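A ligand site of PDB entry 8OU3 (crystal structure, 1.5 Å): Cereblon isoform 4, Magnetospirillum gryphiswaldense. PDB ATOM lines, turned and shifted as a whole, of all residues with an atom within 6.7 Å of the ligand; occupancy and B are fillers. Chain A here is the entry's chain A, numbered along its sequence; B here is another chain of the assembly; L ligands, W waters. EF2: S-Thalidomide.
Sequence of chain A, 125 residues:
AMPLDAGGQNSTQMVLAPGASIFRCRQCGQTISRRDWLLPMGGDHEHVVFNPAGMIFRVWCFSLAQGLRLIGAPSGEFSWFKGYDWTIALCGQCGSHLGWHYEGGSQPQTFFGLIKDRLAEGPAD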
ATOM      1  N   VAL A  49       0.042  -5.629 -10.964  1.00  0.00           N
ATOM      2  CA  VAL A  49      -0.085  -4.951  -9.689  1.00  0.00           C
ATOM      3  C   VAL A  49       1.256  -4.867  -8.976  1.00  0.00           C
ATOM      4  O   VAL A  49       2.157  -5.632  -9.288  1.00  0.00           O
ATOM      5  CB  VAL A  49      -1.107  -5.715  -8.824  1.00  0.00           C
ATOM      6  CG1 VAL A  49      -2.480  -5.684  -9.476  1.00  0.00           C
ATOM      7  CG2 VAL A  49      -0.686  -7.151  -8.522  1.00  0.00           C
ATOM      8  N   PHE A  50       1.383  -3.949  -7.989  1.00  0.00           N
ATOM      9  CA  PHE A  50       2.554  -3.982  -7.124  1.00  0.00           C
ATOM     10  C   PHE A  50       2.175  -3.893  -5.653  1.00  0.00           C
ATOM     11  O   PHE A  50       1.136  -3.334  -5.293  1.00  0.00           O
ATOM     12  CB  PHE A  50       3.606  -2.928  -7.522  1.00  0.00           C
ATOM     13  CG  PHE A  50       3.161  -1.520  -7.367  1.00  0.00           C
ATOM     14  CD1 PHE A  50       2.411  -0.891  -8.366  1.00  0.00           C
ATOM     15  CD2 PHE A  50       3.457  -0.803  -6.209  1.00  0.00           C
ATOM     16  CE1 PHE A  50       2.002   0.419  -8.196  1.00  0.00           C
ATOM     17  CE2 PHE A  50       3.049   0.506  -6.052  1.00  0.00           C
ATOM     18  CZ  PHE A  50       2.306   1.116  -7.042  1.00  0.00           C
ATOM     19  N   ASN A  51       2.983  -4.562  -4.833  1.00  0.00           N
ATOM     20  CA  ASN A  51       2.811  -4.514  -3.402  1.00  0.00           C
ATOM     21  C   ASN A  51       3.575  -3.356  -2.760  1.00  0.00           C
ATOM     22  O   ASN A  51       4.274  -2.556  -3.427  1.00  0.00           O
ATOM     23  CB  ASN A  51       3.110  -5.884  -2.805  1.00  0.00           C
ATOM     24  CG  ASN A  51       4.581  -6.260  -2.831  1.00  0.00           C
ATOM     25  OD1 ASN A  51       5.465  -5.417  -3.033  1.00  0.00           O
ATOM     26  ND2 ASN A  51       4.831  -7.463  -2.363  1.00  0.00           N
ATOM     27  N   PRO A  52       3.416  -3.139  -1.435  1.00  0.00           N
ATOM     28  CA  PRO A  52       4.112  -2.057  -0.768  1.00  0.00           C
ATOM     29  C   PRO A  52       5.642  -2.130  -0.782  1.00  0.00           C
ATOM     30  O   PRO A  52       6.270  -1.088  -0.597  1.00  0.00           O
ATOM     31  CB  PRO A  52       3.568  -2.099   0.672  1.00  0.00           C
ATOM     32  CG  PRO A  52       2.224  -2.846   0.560  1.00  0.00           C
ATOM     33  CD  PRO A  52       2.440  -3.825  -0.560  1.00  0.00           C
ATOM     34  N   ALA A  53       6.183  -3.337  -1.013  1.00  0.00           N
ATOM     35  CA  ALA A  53       7.618  -3.527  -1.169  1.00  0.00           C
ATOM     36  C   ALA A  53       8.047  -3.317  -2.627  1.00  0.00           C
ATOM     37  O   ALA A  53       9.212  -3.554  -2.952  1.00  0.00           O
ATOM     38  CB  ALA A  53       8.026  -4.872  -0.663  1.00  0.00           C
ATOM     39  N   MET A  55       7.273  -4.863  -5.360  1.00  0.00           N
ATOM     40  CA  MET A  55       7.266  -6.050  -6.215  1.00  0.00           C
ATOM     41  C   MET A  55       6.100  -5.972  -7.176  1.00  0.00           C
ATOM     42  O   MET A  55       4.944  -5.759  -6.743  1.00  0.00           O
ATOM     43  CB  MET A  55       7.240  -7.346  -5.415  1.00  0.00           C
ATOM     44  CG  MET A  55       8.384  -7.455  -4.445  1.00  0.00           C
ATOM     45  SD  MET A  55       8.277  -8.823  -3.286  1.00  0.00           S
ATOM     46  CE  MET A  55       9.653  -8.375  -2.219  1.00  0.00           C
ATOM     47  N   PHE A  57       3.718  -7.923  -9.923  1.00  0.00           N
ATOM     48  CA  PHE A  57       3.191  -9.269 -10.115  1.00  0.00           C
ATOM     49  C   PHE A  57       2.249  -9.244 -11.313  1.00  0.00           C
ATOM     50  O   PHE A  57       1.403  -8.364 -11.434  1.00  0.00           O
ATOM     51  CB  PHE A  57       2.435  -9.803  -8.883  1.00  0.00           C
ATOM     52  CG  PHE A  57       3.193  -9.878  -7.581  1.00  0.00           C
ATOM     53  CD1 PHE A  57       4.046 -10.923  -7.304  1.00  0.00           C
ATOM     54  CD2 PHE A  57       3.122  -8.857  -6.651  1.00  0.00           C
ATOM     55  CE1 PHE A  57       4.739 -10.993  -6.097  1.00  0.00           C
ATOM     56  CE2 PHE A  57       3.830  -8.938  -5.457  1.00  0.00           C
ATOM     57  CZ  PHE A  57       4.636 -10.000  -5.180  1.00  0.00           C
ATOM     58  N   SER A  75      -7.237 -10.421   5.237  1.00  0.00           N
ATOM     59  CA  SER A  75      -6.931  -9.026   5.439  1.00  0.00           C
ATOM     60  C   SER A  75      -7.406  -8.217   4.243  1.00  0.00           C
ATOM     61  O   SER A  75      -7.231  -8.651   3.120  1.00  0.00           O
ATOM     62  CB  SER A  75      -5.435  -8.807   5.614  1.00  0.00           C
ATOM     63  OG  SER A  75      -5.214  -7.413   5.827  1.00  0.00           O
ATOM     64  N   GLU A  77      -6.130  -5.081   3.882  1.00  0.00           N
ATOM     65  CA  GLU A  77      -5.118  -4.036   3.710  1.00  0.00           C
ATOM     66  C   GLU A  77      -4.442  -4.180   2.346  1.00  0.00           C
ATOM     67  O   GLU A  77      -4.017  -5.244   1.986  1.00  0.00           O
ATOM     68  CB  GLU A  77      -4.104  -4.138   4.853  1.00  0.00           C
ATOM     69  CG  GLU A  77      -4.772  -3.873   6.193  1.00  0.00           C
ATOM     70  CD  GLU A  77      -3.891  -3.818   7.432  1.00  0.00           C
ATOM     71  OE1 GLU A  77      -2.755  -4.327   7.384  1.00  0.00           O
ATOM     72  OE2 GLU A  77      -4.361  -3.247   8.435  1.00  0.00           O
ATOM     73  N   PHE A  78      -4.403  -3.064   1.583  1.00  0.00           N
ATOM     74  CA  PHE A  78      -3.688  -2.996   0.309  1.00  0.00           C
ATOM     75  C   PHE A  78      -4.327  -3.883  -0.755  1.00  0.00           C
ATOM     76  O   PHE A  78      -3.711  -4.212  -1.765  1.00  0.00           O
ATOM     77  CB  PHE A  78      -2.206  -3.374   0.461  1.00  0.00           C
ATOM     78  CG  PHE A  78      -1.437  -2.579   1.494  1.00  0.00           C
ATOM     79  CD1 PHE A  78      -1.185  -1.265   1.282  1.00  0.00           C
ATOM     80  CD2 PHE A  78      -0.934  -3.203   2.619  1.00  0.00           C
ATOM     81  CE1 PHE A  78      -0.483  -0.518   2.218  1.00  0.00           C
ATOM     82  CE2 PHE A  78      -0.230  -2.463   3.562  1.00  0.00           C
ATOM     83  CZ  PHE A  78       0.023  -1.150   3.336  1.00  0.00           C
ATOM     84  N   SER A  79      -5.555  -4.369  -0.550  1.00  0.00           N
ATOM     85  CA  SER A  79      -6.126  -5.268  -1.526  1.00  0.00           C
ATOM     86  C   SER A  79      -6.211  -4.619  -2.909  1.00  0.00           C
ATOM     87  O   SER A  79      -6.652  -3.478  -3.045  1.00  0.00           O
ATOM     88  CB  SER A  79      -7.548  -5.665  -1.144  1.00  0.00           C
ATOM     89  OG  SER A  79      -8.006  -6.611  -2.098  1.00  0.00           O
ATOM     90  N   TRP A  80      -5.787  -5.412  -3.916  1.00  0.00           N
ATOM     91  CA  TRP A  80      -5.812  -4.985  -5.308  1.00  0.00           C
ATOM     92  C   TRP A  80      -7.211  -5.057  -5.917  1.00  0.00           C
ATOM     93  O   TRP A  80      -7.422  -4.503  -6.998  1.00  0.00           O
ATOM     94  CB  TRP A  80      -4.827  -5.797  -6.138  1.00  0.00           C
ATOM     95  CG  TRP A  80      -3.387  -5.602  -5.758  1.00  0.00           C
ATOM     96  CD1 TRP A  80      -2.724  -4.424  -5.555  1.00  0.00           C
ATOM     97  CD2 TRP A  80      -2.455  -6.659  -5.527  1.00  0.00           C
ATOM     98  NE1 TRP A  80      -1.403  -4.688  -5.254  1.00  0.00           N
ATOM     99  CE2 TRP A  80      -1.214  -6.039  -5.238  1.00  0.00           C
ATOM    100  CE3 TRP A  80      -2.517  -8.053  -5.551  1.00  0.00           C
ATOM    101  CZ2 TRP A  80      -0.074  -6.793  -4.932  1.00  0.00           C
ATOM    102  CZ3 TRP A  80      -1.395  -8.788  -5.290  1.00  0.00           C
ATOM    103  CH2 TRP A  80      -0.193  -8.148  -4.961  1.00  0.00           C
ATOM    104  N   PHE A  81      -8.158  -5.704  -5.229  1.00  0.00           N
ATOM    105  CA  PHE A  81      -9.466  -5.936  -5.793  1.00  0.00           C
ATOM    106  C   PHE A  81     -10.519  -5.431  -4.819  1.00  0.00           C
ATOM    107  O   PHE A  81     -10.609  -5.951  -3.715  1.00  0.00           O
ATOM    108  CB  PHE A  81      -9.663  -7.424  -6.126  1.00  0.00           C
ATOM    109  CG  PHE A  81      -8.663  -7.987  -7.104  1.00  0.00           C
ATOM    110  CD1 PHE A  81      -8.874  -7.837  -8.465  1.00  0.00           C
ATOM    111  CD2 PHE A  81      -7.555  -8.658  -6.672  1.00  0.00           C
ATOM    112  CE1 PHE A  81      -8.019  -8.440  -9.381  1.00  0.00           C
ATOM    113  CE2 PHE A  81      -6.652  -9.189  -7.571  1.00  0.00           C
ATOM    114  CZ  PHE A  81      -6.876  -9.059  -8.931  1.00  0.00           C
ATOM    115  N   TYR A  84     -12.642  -7.136  -1.678  1.00  0.00           N
ATOM    116  CA  TYR A  84     -12.121  -8.437  -1.300  1.00  0.00           C
ATOM    117  C   TYR A  84     -11.010  -8.340  -0.276  1.00  0.00           C
ATOM    118  O   TYR A  84     -10.207  -7.395  -0.284  1.00  0.00           O
ATOM    119  CB  TYR A  84     -11.580  -9.169  -2.528  1.00  0.00           C
ATOM    120  CG  TYR A  84     -12.618  -9.468  -3.575  1.00  0.00           C
ATOM    121  CD1 TYR A  84     -13.331 -10.657  -3.538  1.00  0.00           C
ATOM    122  CD2 TYR A  84     -12.846  -8.606  -4.618  1.00  0.00           C
ATOM    123  CE1 TYR A  84     -14.289 -10.940  -4.491  1.00  0.00           C
ATOM    124  CE2 TYR A  84     -13.837  -8.856  -5.575  1.00  0.00           C
ATOM    125  CZ  TYR A  84     -14.539 -10.047  -5.516  1.00  0.00           C
ATOM    126  OH  TYR A  84     -15.503 -10.285  -6.459  1.00  0.00           O
ATOM    127  N   TRP A  86      -7.824 -10.727   1.459  1.00  0.00           N
ATOM    128  CA  TRP A  86      -6.913 -11.721   0.910  1.00  0.00           C
ATOM    129  C   TRP A  86      -6.245 -12.560   2.002  1.00  0.00           C
ATOM    130  O   TRP A  86      -6.043 -12.079   3.119  1.00  0.00           O
ATOM    131  CB  TRP A  86      -5.862 -11.062   0.019  1.00  0.00           C
ATOM    132  CG  TRP A  86      -5.114  -9.947   0.670  1.00  0.00           C
ATOM    133  CD1 TRP A  86      -5.388  -8.625   0.589  1.00  0.00           C
ATOM    134  CD2 TRP A  86      -3.966 -10.063   1.542  1.00  0.00           C
ATOM    135  NE1 TRP A  86      -4.505  -7.904   1.348  1.00  0.00           N
ATOM    136  CE2 TRP A  86      -3.660  -8.759   1.985  1.00  0.00           C
ATOM    137  CE3 TRP A  86      -3.219 -11.141   2.031  1.00  0.00           C
ATOM    138  CZ2 TRP A  86      -2.614  -8.510   2.873  1.00  0.00           C
ATOM    139  CZ3 TRP A  86      -2.175 -10.888   2.897  1.00  0.00           C
ATOM    140  CH2 TRP A  86      -1.877  -9.589   3.313  1.00  0.00           C
ATOM    141  N   ILE A  88      -2.661 -15.172   1.944  1.00  0.00           N
ATOM    142  CA  ILE A  88      -1.552 -15.744   1.176  1.00  0.00           C
ATOM    143  C   ILE A  88      -1.871 -17.190   0.793  1.00  0.00           C
ATOM    144  O   ILE A  88      -2.304 -18.018   1.648  1.00  0.00           O
ATOM    145  CB  ILE A  88      -0.257 -15.623   1.983  1.00  0.00           C
ATOM    146  CG1 ILE A  88       0.101 -14.139   2.123  1.00  0.00           C
ATOM    147  CG2 ILE A  88       0.876 -16.435   1.371  1.00  0.00           C
ATOM    148  CD1 ILE A  88       1.251 -13.883   3.078  1.00  0.00           C
ATOM    149  N   HIS A  97       5.392 -19.366  -2.768  1.00  0.00           N
ATOM    150  CA  HIS A  97       4.287 -18.422  -2.711  1.00  0.00           C
ATOM    151  C   HIS A  97       3.676 -18.225  -4.104  1.00  0.00           C
ATOM    152  O   HIS A  97       4.319 -17.648  -4.995  1.00  0.00           O
ATOM    153  CB  HIS A  97       4.748 -17.074  -2.174  1.00  0.00           C
ATOM    154  CG  HIS A  97       3.696 -16.043  -2.208  1.00  0.00           C
ATOM    155  ND1 HIS A  97       3.984 -14.681  -2.287  1.00  0.00           N
ATOM    156  CD2 HIS A  97       2.362 -16.153  -2.095  1.00  0.00           C
ATOM    157  CE1 HIS A  97       2.843 -14.017  -2.259  1.00  0.00           C
ATOM    158  NE2 HIS A  97       1.842 -14.888  -2.137  1.00  0.00           N
ATOM    159  N   TRP A 100      -2.649 -15.463  -3.952  1.00  0.00           N
ATOM    160  CA  TRP A 100      -3.555 -15.097  -2.869  1.00  0.00           C
ATOM    161  C   TRP A 100      -4.922 -15.695  -3.158  1.00  0.00           C
ATOM    162  O   TRP A 100      -5.331 -15.789  -4.328  1.00  0.00           O
ATOM    163  CB  TRP A 100      -3.628 -13.572  -2.691  1.00  0.00           C
ATOM    164  CG  TRP A 100      -2.289 -12.898  -2.530  1.00  0.00           C
ATOM    165  CD1 TRP A 100      -1.681 -12.593  -1.342  1.00  0.00           C
ATOM    166  CD2 TRP A 100      -1.343 -12.532  -3.557  1.00  0.00           C
ATOM    167  NE1 TRP A 100      -0.433 -12.101  -1.560  1.00  0.00           N
ATOM    168  CE2 TRP A 100      -0.224 -11.990  -2.889  1.00  0.00           C
ATOM    169  CE3 TRP A 100      -1.356 -12.570  -4.953  1.00  0.00           C
ATOM    170  CZ2 TRP A 100       0.901 -11.535  -3.584  1.00  0.00           C
ATOM    171  CZ3 TRP A 100      -0.234 -12.139  -5.653  1.00  0.00           C
ATOM    172  CH2 TRP A 100       0.872 -11.645  -4.967  1.00  0.00           C
ATOM    173  N   TYR A 102      -8.831 -14.665  -2.479  1.00  0.00           N
ATOM    174  CA  TYR A 102      -9.680 -13.522  -2.195  1.00  0.00           C
ATOM    175  C   TYR A 102     -11.078 -13.982  -1.779  1.00  0.00           C
ATOM    176  O   TYR A 102     -11.624 -14.925  -2.353  1.00  0.00           O
ATOM    177  CB  TYR A 102      -9.740 -12.623  -3.428  1.00  0.00           C
ATOM    178  CG  TYR A 102      -8.434 -11.912  -3.711  1.00  0.00           C
ATOM    179  CD1 TYR A 102      -8.133 -10.740  -3.044  1.00  0.00           C
ATOM    180  CD2 TYR A 102      -7.498 -12.477  -4.542  1.00  0.00           C
ATOM    181  CE1 TYR A 102      -6.915 -10.080  -3.291  1.00  0.00           C
ATOM    182  CE2 TYR A 102      -6.294 -11.838  -4.788  1.00  0.00           C
ATOM    183  CZ  TYR A 102      -5.995 -10.689  -4.112  1.00  0.00           C
ATOM    184  OH  TYR A 102      -4.753 -10.066  -4.369  1.00  0.00           O
ATOM    185  N   GLY B  19      -5.177  -0.519  -2.285  1.00  0.00           N
ATOM    186  CA  GLY B  19      -3.963  -1.001  -2.985  1.00  0.00           C
ATOM    187  C   GLY B  19      -3.912  -0.575  -4.452  1.00  0.00           C
ATOM    188  O   GLY B  19      -3.086  -1.074  -5.200  1.00  0.00           O
ATOM    189  N   PRO B 123      -0.259   0.353  -3.894  1.00  0.00           N
ATOM    190  CA  PRO B 123      -0.551   1.279  -2.793  1.00  0.00           C
ATOM    191  C   PRO B 123       0.318   2.537  -2.795  1.00  0.00           C
ATOM    192  O   PRO B 123       1.413   2.548  -3.348  1.00  0.00           O
ATOM    193  CB  PRO B 123      -0.235   0.438  -1.550  1.00  0.00           C
ATOM    194  CG  PRO B 123       0.794  -0.588  -2.014  1.00  0.00           C
ATOM    195  CD  PRO B 123       0.409  -0.888  -3.458  1.00  0.00           C
HETATM  196  O01 EF2 L   1      -0.378  -5.566  -1.777  1.00  0.00           O
HETATM  197  C02 EF2 L   1      -0.955  -6.633  -1.773  1.00  0.00           C
HETATM  198  N03 EF2 L   1      -2.271  -6.673  -2.198  1.00  0.00           N
HETATM  199  C04 EF2 L   1      -3.068  -7.805  -2.274  1.00  0.00           C
HETATM  200  O05 EF2 L   1      -4.173  -7.723  -2.794  1.00  0.00           O
HETATM  201  C06 EF2 L   1      -2.454  -9.071  -1.803  1.00  0.00           C
HETATM  202  C07 EF2 L   1      -1.421  -8.907  -0.717  1.00  0.00           C
HETATM  203  C08 EF2 L   1      -0.368  -7.913  -1.188  1.00  0.00           C
HETATM  204  N09 EF2 L   1       0.639  -7.591  -0.180  1.00  0.00           N
HETATM  205  C11 EF2 L   1       3.688  -6.208   3.012  1.00  0.00           C
HETATM  206  C12 EF2 L   1       2.321  -6.139   2.740  1.00  0.00           C
HETATM  207  C13 EF2 L   1       1.869  -6.753   1.590  1.00  0.00           C
HETATM  208  C14 EF2 L   1       2.748  -7.452   0.774  1.00  0.00           C
HETATM  209  O16 EF2 L   1      -0.543  -6.393   1.429  1.00  0.00           O
HETATM  210  O18 EF2 L   1       2.372  -8.638  -1.293  1.00  0.00           O
HETATM  211  C19 EF2 L   1       4.099  -7.535   1.040  1.00  0.00           C
HETATM  212  C20 EF2 L   1       4.565  -6.902   2.175  1.00  0.00           C
HETATM  213  C3  EF2 L   1       1.969  -7.989  -0.365  1.00  0.00           C
HETATM  214  C4  EF2 L   1       0.493  -6.860   1.013  1.00  0.00           C
HETATM  215  O   HOH W   1       1.420 -11.106   0.573  1.00  0.00           O
HETATM  216  O   HOH W   2      -0.482  -6.333   4.656  1.00  0.00           O
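The backbone NH (N) of Glu 77 lies within hydrogen-bond range of the side-chain hydroxyl (OG) of Ser 75, 3.2 Å away. O of Tyr 84 sits at hydrogen-bond distance from OG of Ser 79 (3.0 Å). The indole nitrogen (NE1) of Trp 80 lies within hydrogen-bond range of the backbone carbonyl oxygen (O) of Phe 50, at 2.9 Å. O of Ser 79 lies within hydrogen-bond range of N of Gly 19 of chain B (3.4 Å). O of Glu 77 lies within hydrogen-bond range of NE1 of Trp 86 (2.8 Å). OD1 of Asn 51 sits at hydrogen-bond distance from N of Met 55. The backbone carbonyl oxygen (O) of Phe 81 sits at hydrogen-bond distance from the side-chain hydroxyl (OG) of Ser 79. The backbone NH (N) of Ala 53 lies within hydrogen-bond range of the side-chain amide oxygen (OD1) of Asn 51, at 3.0 Å.
CD of Pro 52 touches O01 of the ligand (3.5 Å). Glu 77 touches the ligand. Ser 79 touches the ligand (CA to O05, 3.4 Å). CZ2 of Trp 86 touches O16 of the ligand, 3.3 Å away. Trp 100 touches the ligand (NE1 to C07, 3.4 Å). Hydrophobic or aromatic side chains that line the ligand: Pro 52, Phe 78, Trp 80, Trp 86, Trp 100 and Tyr 102.
Water W1 lies within hydrogen-bond range of the indole nitrogen of Trp 100 (3.0 Å) and an oxygen (O18) of the ligand (3.2 Å).
The side-chain hydroxyl of Tyr 102 is in hydrogen-bond range of an oxygen (O05) of the ligand, at 2.9 Å. An oxygen (O05) of the ligand is in hydrogen-bond range of the backbone NH of Trp 80. The side-chain amide nitrogen (ND2) of Asn 51 is in hydrogen-bond range of an oxygen (O18) of the ligand, 2.9 Å away. The backbone carbonyl oxygen of Phe 78 sits at hydrogen-bond distance from a nitrogen (N03) of the ligand (2.9 Å).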
